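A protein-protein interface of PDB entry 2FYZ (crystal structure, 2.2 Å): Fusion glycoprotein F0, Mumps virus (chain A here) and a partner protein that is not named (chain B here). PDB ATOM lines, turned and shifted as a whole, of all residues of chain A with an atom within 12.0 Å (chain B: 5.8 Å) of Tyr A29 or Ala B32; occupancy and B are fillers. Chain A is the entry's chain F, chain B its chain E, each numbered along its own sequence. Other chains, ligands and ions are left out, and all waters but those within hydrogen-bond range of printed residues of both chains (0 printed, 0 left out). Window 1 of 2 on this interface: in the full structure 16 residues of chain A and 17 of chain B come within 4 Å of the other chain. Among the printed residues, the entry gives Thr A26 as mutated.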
ATOM      1  N   LYS A  18     -17.386  -0.851   1.131  1.00  0.00           N
ATOM      2  CA  LYS A  18     -17.720  -1.506   2.392  1.00  0.00           C
ATOM      3  C   LYS A  18     -19.195  -1.897   2.286  1.00  0.00           C
ATOM      4  O   LYS A  18     -19.587  -3.006   2.638  1.00  0.00           O
ATOM      5  CB  LYS A  18     -17.557  -0.545   3.578  1.00  0.00           C
ATOM      6  CG  LYS A  18     -16.166   0.030   3.805  1.00  0.00           C
ATOM      7  CD  LYS A  18     -15.306  -0.910   4.611  1.00  0.00           C
ATOM      8  CE  LYS A  18     -14.010  -0.243   5.060  1.00  0.00           C
ATOM      9  NZ  LYS A  18     -14.233   0.860   6.033  1.00  0.00           N
ATOM     10  N   VAL A  19     -20.007  -0.958   1.806  1.00  0.00           N
ATOM     11  CA  VAL A  19     -21.444  -1.172   1.651  1.00  0.00           C
ATOM     12  C   VAL A  19     -21.725  -2.422   0.832  1.00  0.00           C
ATOM     13  O   VAL A  19     -22.470  -3.313   1.254  1.00  0.00           O
ATOM     14  CB  VAL A  19     -22.118   0.031   0.929  1.00  0.00           C
ATOM     15  CG1 VAL A  19     -23.566  -0.303   0.582  1.00  0.00           C
ATOM     16  CG2 VAL A  19     -22.053   1.271   1.807  1.00  0.00           C
ATOM     17  N   ASN A  20     -21.121  -2.467  -0.350  1.00  0.00           N
ATOM     18  CA  ASN A  20     -21.301  -3.579  -1.271  1.00  0.00           C
ATOM     19  C   ASN A  20     -20.867  -4.918  -0.675  1.00  0.00           C
ATOM     20  O   ASN A  20     -21.482  -5.955  -0.944  1.00  0.00           O
ATOM     21  CB  ASN A  20     -20.537  -3.297  -2.568  1.00  0.00           C
ATOM     22  CG  ASN A  20     -20.639  -4.440  -3.561  1.00  0.00           C
ATOM     23  OD1 ASN A  20     -19.933  -5.440  -3.447  1.00  0.00           O
ATOM     24  ND2 ASN A  20     -21.537  -4.305  -4.533  1.00  0.00           N
ATOM     25  N   ALA A  21     -19.811  -4.897   0.134  1.00  0.00           N
ATOM     26  CA  ALA A  21     -19.329  -6.126   0.761  1.00  0.00           C
ATOM     27  C   ALA A  21     -20.345  -6.598   1.796  1.00  0.00           C
ATOM     28  O   ALA A  21     -20.591  -7.795   1.940  1.00  0.00           O
ATOM     29  CB  ALA A  21     -17.981  -5.889   1.425  1.00  0.00           C
ATOM     30  N   SER A  22     -20.931  -5.652   2.523  1.00  0.00           N
ATOM     31  CA  SER A  22     -21.928  -5.995   3.526  1.00  0.00           C
ATOM     32  C   SER A  22     -23.133  -6.633   2.845  1.00  0.00           C
ATOM     33  O   SER A  22     -23.632  -7.675   3.280  1.00  0.00           O
ATOM     34  CB  SER A  22     -22.378  -4.744   4.287  1.00  0.00           C
ATOM     35  OG  SER A  22     -21.308  -4.170   5.020  1.00  0.00           O
ATOM     36  N   LEU A  23     -23.600  -6.000   1.774  1.00  0.00           N
ATOM     37  CA  LEU A  23     -24.753  -6.505   1.049  1.00  0.00           C
ATOM     38  C   LEU A  23     -24.509  -7.897   0.478  1.00  0.00           C
ATOM     39  O   LEU A  23     -25.412  -8.733   0.461  1.00  0.00           O
ATOM     40  CB  LEU A  23     -25.146  -5.525  -0.061  1.00  0.00           C
ATOM     41  CG  LEU A  23     -25.494  -4.136   0.488  1.00  0.00           C
ATOM     42  CD1 LEU A  23     -26.077  -3.246  -0.617  1.00  0.00           C
ATOM     43  CD2 LEU A  23     -26.495  -4.284   1.640  1.00  0.00           C
ATOM     44  N   GLN A  24     -23.292  -8.151   0.014  1.00  0.00           N
ATOM     45  CA  GLN A  24     -22.972  -9.464  -0.524  1.00  0.00           C
ATOM     46  C   GLN A  24     -22.971 -10.452   0.629  1.00  0.00           C
ATOM     47  O   GLN A  24     -23.338 -11.611   0.465  1.00  0.00           O
ATOM     48  CB  GLN A  24     -21.604  -9.450  -1.209  1.00  0.00           C
ATOM     49  CG  GLN A  24     -21.570  -8.596  -2.459  1.00  0.00           C
ATOM     50  CD  GLN A  24     -20.170  -8.440  -3.022  1.00  0.00           C
ATOM     51  OE1 GLN A  24     -19.275  -7.906  -2.353  1.00  0.00           O
ATOM     52  NE2 GLN A  24     -19.968  -8.904  -4.256  1.00  0.00           N
ATOM     53  N   ASN A  25     -22.559  -9.986   1.802  1.00  0.00           N
ATOM     54  CA  ASN A  25     -22.542 -10.839   2.978  1.00  0.00           C
ATOM     55  C   ASN A  25     -23.981 -11.234   3.338  1.00  0.00           C
ATOM     56  O   ASN A  25     -24.240 -12.358   3.770  1.00  0.00           O
ATOM     57  CB  ASN A  25     -21.895 -10.114   4.151  1.00  0.00           C
ATOM     58  CG  ASN A  25     -20.663 -10.823   4.655  1.00  0.00           C
ATOM     59  OD1 ASN A  25     -19.615 -10.815   4.002  1.00  0.00           O
ATOM     60  ND2 ASN A  25     -20.782 -11.459   5.817  1.00  0.00           N
ATOM     61  N   THR A  26     -24.905 -10.299   3.149  1.00  0.00           N
ATOM     62  CA  THR A  26     -26.317 -10.550   3.423  1.00  0.00           C
ATOM     63  C   THR A  26     -26.827 -11.691   2.558  1.00  0.00           C
ATOM     64  O   THR A  26     -27.488 -12.602   3.060  1.00  0.00           O
ATOM     65  CB  THR A  26     -27.189  -9.330   3.116  1.00  0.00           C
ATOM     66  OG1 THR A  26     -26.934  -8.302   4.072  1.00  0.00           O
ATOM     67  CG2 THR A  26     -28.666  -9.712   3.168  1.00  0.00           C
ATOM     68  N   VAL A  27     -26.532 -11.623   1.257  1.00  0.00           N
ATOM     69  CA  VAL A  27     -26.944 -12.654   0.302  1.00  0.00           C
ATOM     70  C   VAL A  27     -26.353 -13.990   0.746  1.00  0.00           C
ATOM     71  O   VAL A  27     -26.995 -15.033   0.662  1.00  0.00           O
ATOM     72  CB  VAL A  27     -26.449 -12.305  -1.133  1.00  0.00           C
ATOM     73  CG1 VAL A  27     -26.693 -13.466  -2.087  1.00  0.00           C
ATOM     74  CG2 VAL A  27     -27.173 -11.057  -1.638  1.00  0.00           C
ATOM     75  N   LYS A  28     -25.122 -13.950   1.228  1.00  0.00           N
ATOM     76  CA  LYS A  28     -24.468 -15.154   1.709  1.00  0.00           C
ATOM     77  C   LYS A  28     -25.291 -15.766   2.845  1.00  0.00           C
ATOM     78  O   LYS A  28     -25.590 -16.956   2.829  1.00  0.00           O
ATOM     79  CB  LYS A  28     -23.065 -14.821   2.206  1.00  0.00           C
ATOM     80  CG  LYS A  28     -22.346 -15.969   2.889  1.00  0.00           C
ATOM     81  CD  LYS A  28     -21.080 -15.460   3.548  1.00  0.00           C
ATOM     82  CE  LYS A  28     -20.401 -16.530   4.378  1.00  0.00           C
ATOM     83  NZ  LYS A  28     -19.173 -15.991   5.033  1.00  0.00           N
ATOM     84  N   TYR A  29     -25.667 -14.954   3.830  1.00  0.00           N
ATOM     85  CA  TYR A  29     -26.455 -15.469   4.947  1.00  0.00           C
ATOM     86  C   TYR A  29     -27.856 -15.906   4.543  1.00  0.00           C
ATOM     87  O   TYR A  29     -28.371 -16.883   5.081  1.00  0.00           O
ATOM     88  CB  TYR A  29     -26.510 -14.445   6.083  1.00  0.00           C
ATOM     89  CG  TYR A  29     -25.194 -14.353   6.816  1.00  0.00           C
ATOM     90  CD1 TYR A  29     -24.532 -13.138   6.958  1.00  0.00           C
ATOM     91  CD2 TYR A  29     -24.583 -15.502   7.323  1.00  0.00           C
ATOM     92  CE1 TYR A  29     -23.287 -13.066   7.579  1.00  0.00           C
ATOM     93  CE2 TYR A  29     -23.339 -15.444   7.943  1.00  0.00           C
ATOM     94  CZ  TYR A  29     -22.698 -14.225   8.068  1.00  0.00           C
ATOM     95  OH  TYR A  29     -21.463 -14.163   8.671  1.00  0.00           O
ATOM     96  N   ILE A  30     -28.478 -15.189   3.608  1.00  0.00           N
ATOM     97  CA  ILE A  30     -29.795 -15.584   3.145  1.00  0.00           C
ATOM     98  C   ILE A  30     -29.638 -16.983   2.547  1.00  0.00           C
ATOM     99  O   ILE A  30     -30.485 -17.857   2.746  1.00  0.00           O
ATOM    100  CB  ILE A  30     -30.330 -14.646   2.056  1.00  0.00           C
ATOM    101  CG1 ILE A  30     -30.664 -13.278   2.656  1.00  0.00           C
ATOM    102  CG2 ILE A  30     -31.570 -15.267   1.407  1.00  0.00           C
ATOM    103  CD1 ILE A  30     -31.100 -12.247   1.625  1.00  0.00           C
ATOM    104  N   LYS A  31     -28.543 -17.197   1.823  1.00  0.00           N
ATOM    105  CA  LYS A  31     -28.289 -18.503   1.220  1.00  0.00           C
ATOM    106  C   LYS A  31     -28.182 -19.573   2.302  1.00  0.00           C
ATOM    107  O   LYS A  31     -28.823 -20.614   2.214  1.00  0.00           O
ATOM    108  CB  LYS A  31     -27.004 -18.486   0.392  1.00  0.00           C
ATOM    109  CG  LYS A  31     -26.700 -19.823  -0.289  1.00  0.00           C
ATOM    110  CD  LYS A  31     -25.470 -19.723  -1.203  1.00  0.00           C
ATOM    111  CE  LYS A  31     -25.207 -21.016  -1.980  1.00  0.00           C
ATOM    112  NZ  LYS A  31     -24.067 -20.859  -2.940  1.00  0.00           N
ATOM    113  N   GLU A  32     -27.367 -19.310   3.316  1.00  0.00           N
ATOM    114  CA  GLU A  32     -27.205 -20.244   4.425  1.00  0.00           C
ATOM    115  C   GLU A  32     -28.561 -20.489   5.087  1.00  0.00           C
ATOM    116  O   GLU A  32     -28.904 -21.624   5.405  1.00  0.00           O
ATOM    117  CB  GLU A  32     -26.207 -19.690   5.447  1.00  0.00           C
ATOM    118  CG  GLU A  32     -24.754 -19.867   5.030  1.00  0.00           C
ATOM    119  CD  GLU A  32     -23.804 -18.889   5.706  1.00  0.00           C
ATOM    120  OE1 GLU A  32     -23.964 -17.667   5.501  1.00  0.00           O
ATOM    121  OE2 GLU A  32     -22.892 -19.336   6.433  1.00  0.00           O
ATOM    122  N   SER A  33     -29.346 -19.434   5.278  1.00  0.00           N
ATOM    123  CA  SER A  33     -30.657 -19.614   5.895  1.00  0.00           C
ATOM    124  C   SER A  33     -31.545 -20.569   5.094  1.00  0.00           C
ATOM    125  O   SER A  33     -32.182 -21.445   5.669  1.00  0.00           O
ATOM    126  CB  SER A  33     -31.392 -18.284   6.057  1.00  0.00           C
ATOM    127  OG  SER A  33     -32.663 -18.509   6.638  1.00  0.00           O
ATOM    128  N   ASN A  34     -31.586 -20.399   3.777  1.00  0.00           N
ATOM    129  CA  ASN A  34     -32.408 -21.269   2.942  1.00  0.00           C
ATOM    130  C   ASN A  34     -31.836 -22.676   2.866  1.00  0.00           C
ATOM    131  O   ASN A  34     -32.570 -23.642   2.703  1.00  0.00           O
ATOM    132  CB  ASN A  34     -32.545 -20.698   1.534  1.00  0.00           C
ATOM    133  CG  ASN A  34     -33.353 -19.429   1.509  1.00  0.00           C
ATOM    134  OD1 ASN A  34     -34.360 -19.313   2.208  1.00  0.00           O
ATOM    135  ND2 ASN A  34     -32.929 -18.468   0.697  1.00  0.00           N
ATOM    136  N   HIS A  35     -30.523 -22.791   2.982  1.00  0.00           N
ATOM    137  CA  HIS A  35     -29.889 -24.100   2.938  1.00  0.00           C
ATOM    138  C   HIS A  35     -30.304 -24.898   4.162  1.00  0.00           C
ATOM    139  O   HIS A  35     -30.517 -26.109   4.083  1.00  0.00           O
ATOM    140  CB  HIS A  35     -28.369 -23.970   2.922  1.00  0.00           C
ATOM    141  CG  HIS A  35     -27.664 -25.283   3.044  1.00  0.00           C
ATOM    142  ND1 HIS A  35     -27.652 -26.216   2.029  1.00  0.00           N
ATOM    143  CD2 HIS A  35     -26.999 -25.847   4.081  1.00  0.00           C
ATOM    144  CE1 HIS A  35     -27.010 -27.295   2.437  1.00  0.00           C
ATOM    145  NE2 HIS A  35     -26.604 -27.097   3.679  1.00  0.00           N
ATOM    146  N   GLN A  36     -30.415 -24.215   5.298  1.00  0.00           N
ATOM    147  CA  GLN A  36     -30.825 -24.864   6.538  1.00  0.00           C
ATOM    148  C   GLN A  36     -32.275 -25.320   6.474  1.00  0.00           C
ATOM    149  O   GLN A  36     -32.629 -26.364   7.030  1.00  0.00           O
ATOM    150  CB  GLN A  36     -30.639 -23.922   7.729  1.00  0.00           C
ATOM    151  CG  GLN A  36     -29.187 -23.691   8.119  1.00  0.00           C
ATOM    152  CD  GLN A  36     -28.491 -24.972   8.557  1.00  0.00           C
ATOM    153  OE1 GLN A  36     -29.008 -25.720   9.386  1.00  0.00           O
ATOM    154  NE2 GLN A  36     -27.312 -25.223   8.005  1.00  0.00           N
ATOM    155  N   LEU A  37     -33.115 -24.541   5.794  1.00  0.00           N
ATOM    156  CA  LEU A  37     -34.527 -24.889   5.677  1.00  0.00           C
ATOM    157  C   LEU A  37     -34.733 -26.127   4.808  1.00  0.00           C
ATOM    158  O   LEU A  37     -35.824 -26.682   4.768  1.00  0.00           O
ATOM    159  CB  LEU A  37     -35.323 -23.706   5.123  1.00  0.00           C
ATOM    160  CG  LEU A  37     -35.338 -22.486   6.056  1.00  0.00           C
ATOM    161  CD1 LEU A  37     -36.012 -21.317   5.359  1.00  0.00           C
ATOM    162  CD2 LEU A  37     -36.059 -22.833   7.362  1.00  0.00           C
ATOM    163  N   GLN A  38     -33.686 -26.547   4.103  1.00  0.00           N
ATOM    164  CA  GLN A  38     -33.764 -27.744   3.272  1.00  0.00           C
ATOM    165  C   GLN A  38     -33.762 -28.982   4.170  1.00  0.00           C
ATOM    166  O   GLN A  38     -34.033 -30.092   3.707  1.00  0.00           O
ATOM    167  CB  GLN A  38     -32.587 -27.809   2.293  1.00  0.00           C
ATOM    168  CG  GLN A  38     -32.848 -27.098   0.966  1.00  0.00           C
ATOM    169  CD  GLN A  38     -31.617 -27.019   0.064  1.00  0.00           C
ATOM    170  OE1 GLN A  38     -30.723 -27.881   0.111  1.00  0.00           O
ATOM    171  NE2 GLN A  38     -31.578 -25.994  -0.778  1.00  0.00           N
ATOM    172  N   GLN B  27     -31.107 -17.934  12.791  1.00  0.00           N
ATOM    173  CA  GLN B  27     -29.850 -17.292  13.155  1.00  0.00           C
ATOM    174  C   GLN B  27     -29.118 -16.777  11.908  1.00  0.00           C
ATOM    175  O   GLN B  27     -28.515 -15.705  11.928  1.00  0.00           O
ATOM    176  CB  GLN B  27     -28.956 -18.271  13.928  1.00  0.00           C
ATOM    177  CG  GLN B  27     -29.407 -18.514  15.368  1.00  0.00           C
ATOM    178  CD  GLN B  27     -28.599 -19.604  16.065  1.00  0.00           C
ATOM    179  OE1 GLN B  27     -28.629 -19.731  17.288  1.00  0.00           O
ATOM    180  NE2 GLN B  27     -27.885 -20.400  15.284  1.00  0.00           N
ATOM    181  N   ALA B  28     -29.175 -17.537  10.819  1.00  0.00           N
ATOM    182  CA  ALA B  28     -28.507 -17.108   9.604  1.00  0.00           C
ATOM    183  C   ALA B  28     -29.273 -15.917   9.025  1.00  0.00           C
ATOM    184  O   ALA B  28     -28.685 -15.001   8.446  1.00  0.00           O
ATOM    185  CB  ALA B  28     -28.438 -18.255   8.601  1.00  0.00           C
ATOM    186  N   THR B  29     -30.585 -15.914   9.206  1.00  0.00           N
ATOM    187  CA  THR B  29     -31.387 -14.812   8.699  1.00  0.00           C
ATOM    188  C   THR B  29     -31.104 -13.540   9.495  1.00  0.00           C
ATOM    189  O   THR B  29     -31.064 -12.449   8.930  1.00  0.00           O
ATOM    190  CB  THR B  29     -32.876 -15.141   8.772  1.00  0.00           C
ATOM    191  OG1 THR B  29     -33.165 -16.184   7.837  1.00  0.00           O
ATOM    192  CG2 THR B  29     -33.717 -13.915   8.447  1.00  0.00           C
ATOM    193  N   ASN B  30     -30.906 -13.680  10.806  1.00  0.00           N
ATOM    194  CA  ASN B  30     -30.613 -12.513  11.627  1.00  0.00           C
ATOM    195  C   ASN B  30     -29.278 -11.924  11.205  1.00  0.00           C
ATOM    196  O   ASN B  30     -29.109 -10.707  11.195  1.00  0.00           O
ATOM    197  CB  ASN B  30     -30.571 -12.870  13.117  1.00  0.00           C
ATOM    198  CG  ASN B  30     -31.941 -13.175  13.679  1.00  0.00           C
ATOM    199  OD1 ASN B  30     -32.944 -12.652  13.194  1.00  0.00           O
ATOM    200  ND2 ASN B  30     -31.992 -14.009  14.717  1.00  0.00           N
ATOM    201  N   ARG B  31     -28.327 -12.791  10.862  1.00  0.00           N
ATOM    202  CA  ARG B  31     -27.019 -12.323  10.422  1.00  0.00           C
ATOM    203  C   ARG B  31     -27.161 -11.539   9.114  1.00  0.00           C
ATOM    204  O   ARG B  31     -26.518 -10.512   8.926  1.00  0.00           O
ATOM    205  CB  ARG B  31     -26.063 -13.508  10.241  1.00  0.00           C
ATOM    206  CG  ARG B  31     -25.416 -13.981  11.543  1.00  0.00           C
ATOM    207  CD  ARG B  31     -24.729 -15.329  11.380  1.00  0.00           C
ATOM    208  NE  ARG B  31     -25.683 -16.425  11.541  1.00  0.00           N
ATOM    209  CZ  ARG B  31     -25.438 -17.698  11.247  1.00  0.00           C
ATOM    210  NH1 ARG B  31     -24.258 -18.065  10.766  1.00  0.00           N
ATOM    211  NH2 ARG B  31     -26.384 -18.607  11.426  1.00  0.00           N
ATOM    212  N   ALA B  32     -28.009 -12.023   8.217  1.00  0.00           N
ATOM    213  CA  ALA B  32     -28.231 -11.330   6.948  1.00  0.00           C
ATOM    214  C   ALA B  32     -28.853  -9.958   7.219  1.00  0.00           C
ATOM    215  O   ALA B  32     -28.464  -8.966   6.611  1.00  0.00           O
ATOM    216  CB  ALA B  32     -29.140 -12.161   6.045  1.00  0.00           C
ATOM    217  N   VAL B  33     -29.818  -9.909   8.136  1.00  0.00           N
ATOM    218  CA  VAL B  33     -30.463  -8.651   8.488  1.00  0.00           C
ATOM    219  C   VAL B  33     -29.410  -7.703   9.065  1.00  0.00           C
ATOM    220  O   VAL B  33     -29.385  -6.508   8.742  1.00  0.00           O
ATOM    221  CB  VAL B  33     -31.589  -8.857   9.541  1.00  0.00           C
ATOM    222  CG1 VAL B  33     -32.184  -7.505   9.949  1.00  0.00           C
ATOM    223  CG2 VAL B  33     -32.678  -9.763   8.970  1.00  0.00           C
ATOM    224  N   PHE B  34     -28.529  -8.232   9.911  1.00  0.00           N
ATOM    225  CA  PHE B  34     -27.493  -7.383  10.487  1.00  0.00           C
ATOM    226  C   PHE B  34     -26.596  -6.843   9.383  1.00  0.00           C
ATOM    227  O   PHE B  34     -26.175  -5.685   9.428  1.00  0.00           O
ATOM    228  CB  PHE B  34     -26.621  -8.146  11.490  1.00  0.00           C
ATOM    229  CG  PHE B  34     -25.583  -7.280  12.155  1.00  0.00           C
ATOM    230  CD1 PHE B  34     -25.936  -6.431  13.202  1.00  0.00           C
ATOM    231  CD2 PHE B  34     -24.267  -7.273  11.704  1.00  0.00           C
ATOM    232  CE1 PHE B  34     -24.994  -5.581  13.790  1.00  0.00           C
ATOM    233  CE2 PHE B  34     -23.313  -6.428  12.283  1.00  0.00           C
ATOM    234  CZ  PHE B  34     -23.678  -5.581  13.328  1.00  0.00           C
ATOM    235  N   GLU B  35     -26.301  -7.683   8.391  1.00  0.00           N
ATOM    236  CA  GLU B  35     -25.442  -7.257   7.295  1.00  0.00           C
ATOM    237  C   GLU B  35     -26.074  -6.125   6.487  1.00  0.00           C
ATOM    238  O   GLU B  35     -25.386  -5.169   6.120  1.00  0.00           O
ATOM    239  CB  GLU B  35     -25.106  -8.431   6.371  1.00  0.00           C
ATOM    240  CG  GLU B  35     -24.159  -9.453   6.975  1.00  0.00           C
ATOM    241  CD  GLU B  35     -22.829  -8.855   7.421  1.00  0.00           C
ATOM    242  OE1 GLU B  35     -22.278  -7.996   6.699  1.00  0.00           O
ATOM    243  OE2 GLU B  35     -22.330  -9.257   8.493  1.00  0.00           O
ATOM    244  N   VAL B  36     -27.370  -6.228   6.207  1.00  0.00           N
ATOM    245  CA  VAL B  36     -28.038  -5.174   5.462  1.00  0.00           C
ATOM    246  C   VAL B  36     -28.000  -3.890   6.281  1.00  0.00           C
ATOM    247  O   VAL B  36     -27.825  -2.811   5.735  1.00  0.00           O
ATOM    248  CB  VAL B  36     -29.502  -5.529   5.136  1.00  0.00           C
ATOM    249  CG1 VAL B  36     -30.145  -4.392   4.369  1.00  0.00           C
ATOM    250  CG2 VAL B  36     -29.550  -6.785   4.290  1.00  0.00           C
ATOM    251  N   LYS B  37     -28.145  -4.019   7.595  1.00  0.00           N
ATOM    252  CA  LYS B  37     -28.101  -2.866   8.483  1.00  0.00           C
ATOM    253  C   LYS B  37     -26.735  -2.184   8.385  1.00  0.00           C
ATOM    254  O   LYS B  37     -26.637  -0.971   8.198  1.00  0.00           O
ATOM    255  CB  LYS B  37     -28.376  -3.305   9.932  1.00  0.00           C
ATOM    256  CG  LYS B  37     -28.297  -2.178  10.967  1.00  0.00           C
ATOM    257  CD  LYS B  37     -26.894  -2.033  11.532  1.00  0.00           C
ATOM    258  CE  LYS B  37     -26.821  -0.891  12.539  1.00  0.00           C
ATOM    259  NZ  LYS B  37     -25.527  -0.870  13.280  1.00  0.00           N
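The backbone carbonyl oxygen (O) of Gln B27 sits at hydrogen-bond distance from the guanidinium group (NE) of Arg B31 (2.9 Å).
O of Lys A18 sits at hydrogen-bond distance from OG of Ser A22 (3.2 Å).
The side-chain hydroxyl (OG1) of Thr A26 is in hydrogen-bond range of the backbone carbonyl oxygen (O) of Ser A22 (3.5 Å).
The backbone carbonyl oxygen (O) of Ile A30 is in hydrogen-bond range of the side-chain amide nitrogen (ND2) of Asn A34 (3.2 Å).
OG1 of Thr B29 sits at hydrogen-bond distance from OG of Ser A33 (2.7 Å).
The backbone NH (N) of Val B36 is in hydrogen-bond range of the side-chain hydroxyl (OG1) of Thr A26 (3.0 Å).
OG1 of Thr A26 lies within hydrogen-bond range of O of Ala B32 (3.0 Å).
Hydrophobic or aromatic side chains of chain B within 4 Å of the printed part of chain A: Ala B28, Ala B32 and Val B36.
Along chain B the printed residues that touch a printed residue of chain A span positions 28 to 36.
Of the 21 printed residues of chain A, 6 touch a printed residue of chain B.
Printed residues of chain A that touch a printed residue of chain B: Ser A22, Asn A25, Thr A26, Tyr A29, Ile A30 and Ser A33.
Hydrophobic or aromatic side chains of chain A that line the printed part of chain B: Tyr A29 and Ile A30.
Among the printed residues, 12 pairs touch across the chains.
Among the printed residues, merely in contact across the chains: Thr A26 with Glu B35 (2.9 Å), Tyr A29 with Ala B28 (3.3 Å), Asn A25 with Glu B35 (3.3 Å), Tyr A29 with Ala B32 (3.5 Å), Ser A22 with Glu B35 (3.5 Å), Tyr A29 with Arg B31 (3.6 Å), Ser A33 with Ala B28 (3.6 Å), Tyr A29 with Glu B35 (3.7 Å) and Ile A30 with Ala B32 (3.9 Å).
Printed residues of chain B within 4 Å of Ser A22: Glu B35 (3.5 Å).
Tyr A29 touches just these residues of chain B: Ala B28, Arg B31, Ala B32 and Glu B35.
Printed residues of chain B within 4 Å of Ile A30: Ala B32.
Printed residues of chain B within 4 Å of Ser A33: Ala B28 and Thr B29.
Of chain A, only Tyr A29 (3.3 Å) and Ser A33 (3.6 Å) come within 4 Å of Ala B28.
Of the printed residues of chain A, Thr B29 touches Ser A33 (2.7 Å).
No residue of chain A comes within 4 Å of Asn B30.
Of the printed residues of chain A, Arg B31 touches Tyr A29 (3.6 Å).
Of the printed residues of chain A, Ala B32 touches Thr A26 (3.0 Å), Tyr A29 (3.5 Å) and Ile A30 (3.9 Å).
No residue of chain A comes within 4 Å of Val B33.
Of chain A, only Ser A22 (3.5 Å), Asn A25 (3.3 Å), Thr A26 (2.9 Å) and Tyr A29 (3.7 Å) come within 4 Å of Glu B35.
Of chain A, only Thr A26 comes within 4 Å of Val B36.
The nearest residue of chain A that does not touch Ala B32 is Asn A25 (5.2 Å).
The nearest printed residue of chain B that does not touch Ile A30 is Ala B28 (4.8 Å).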
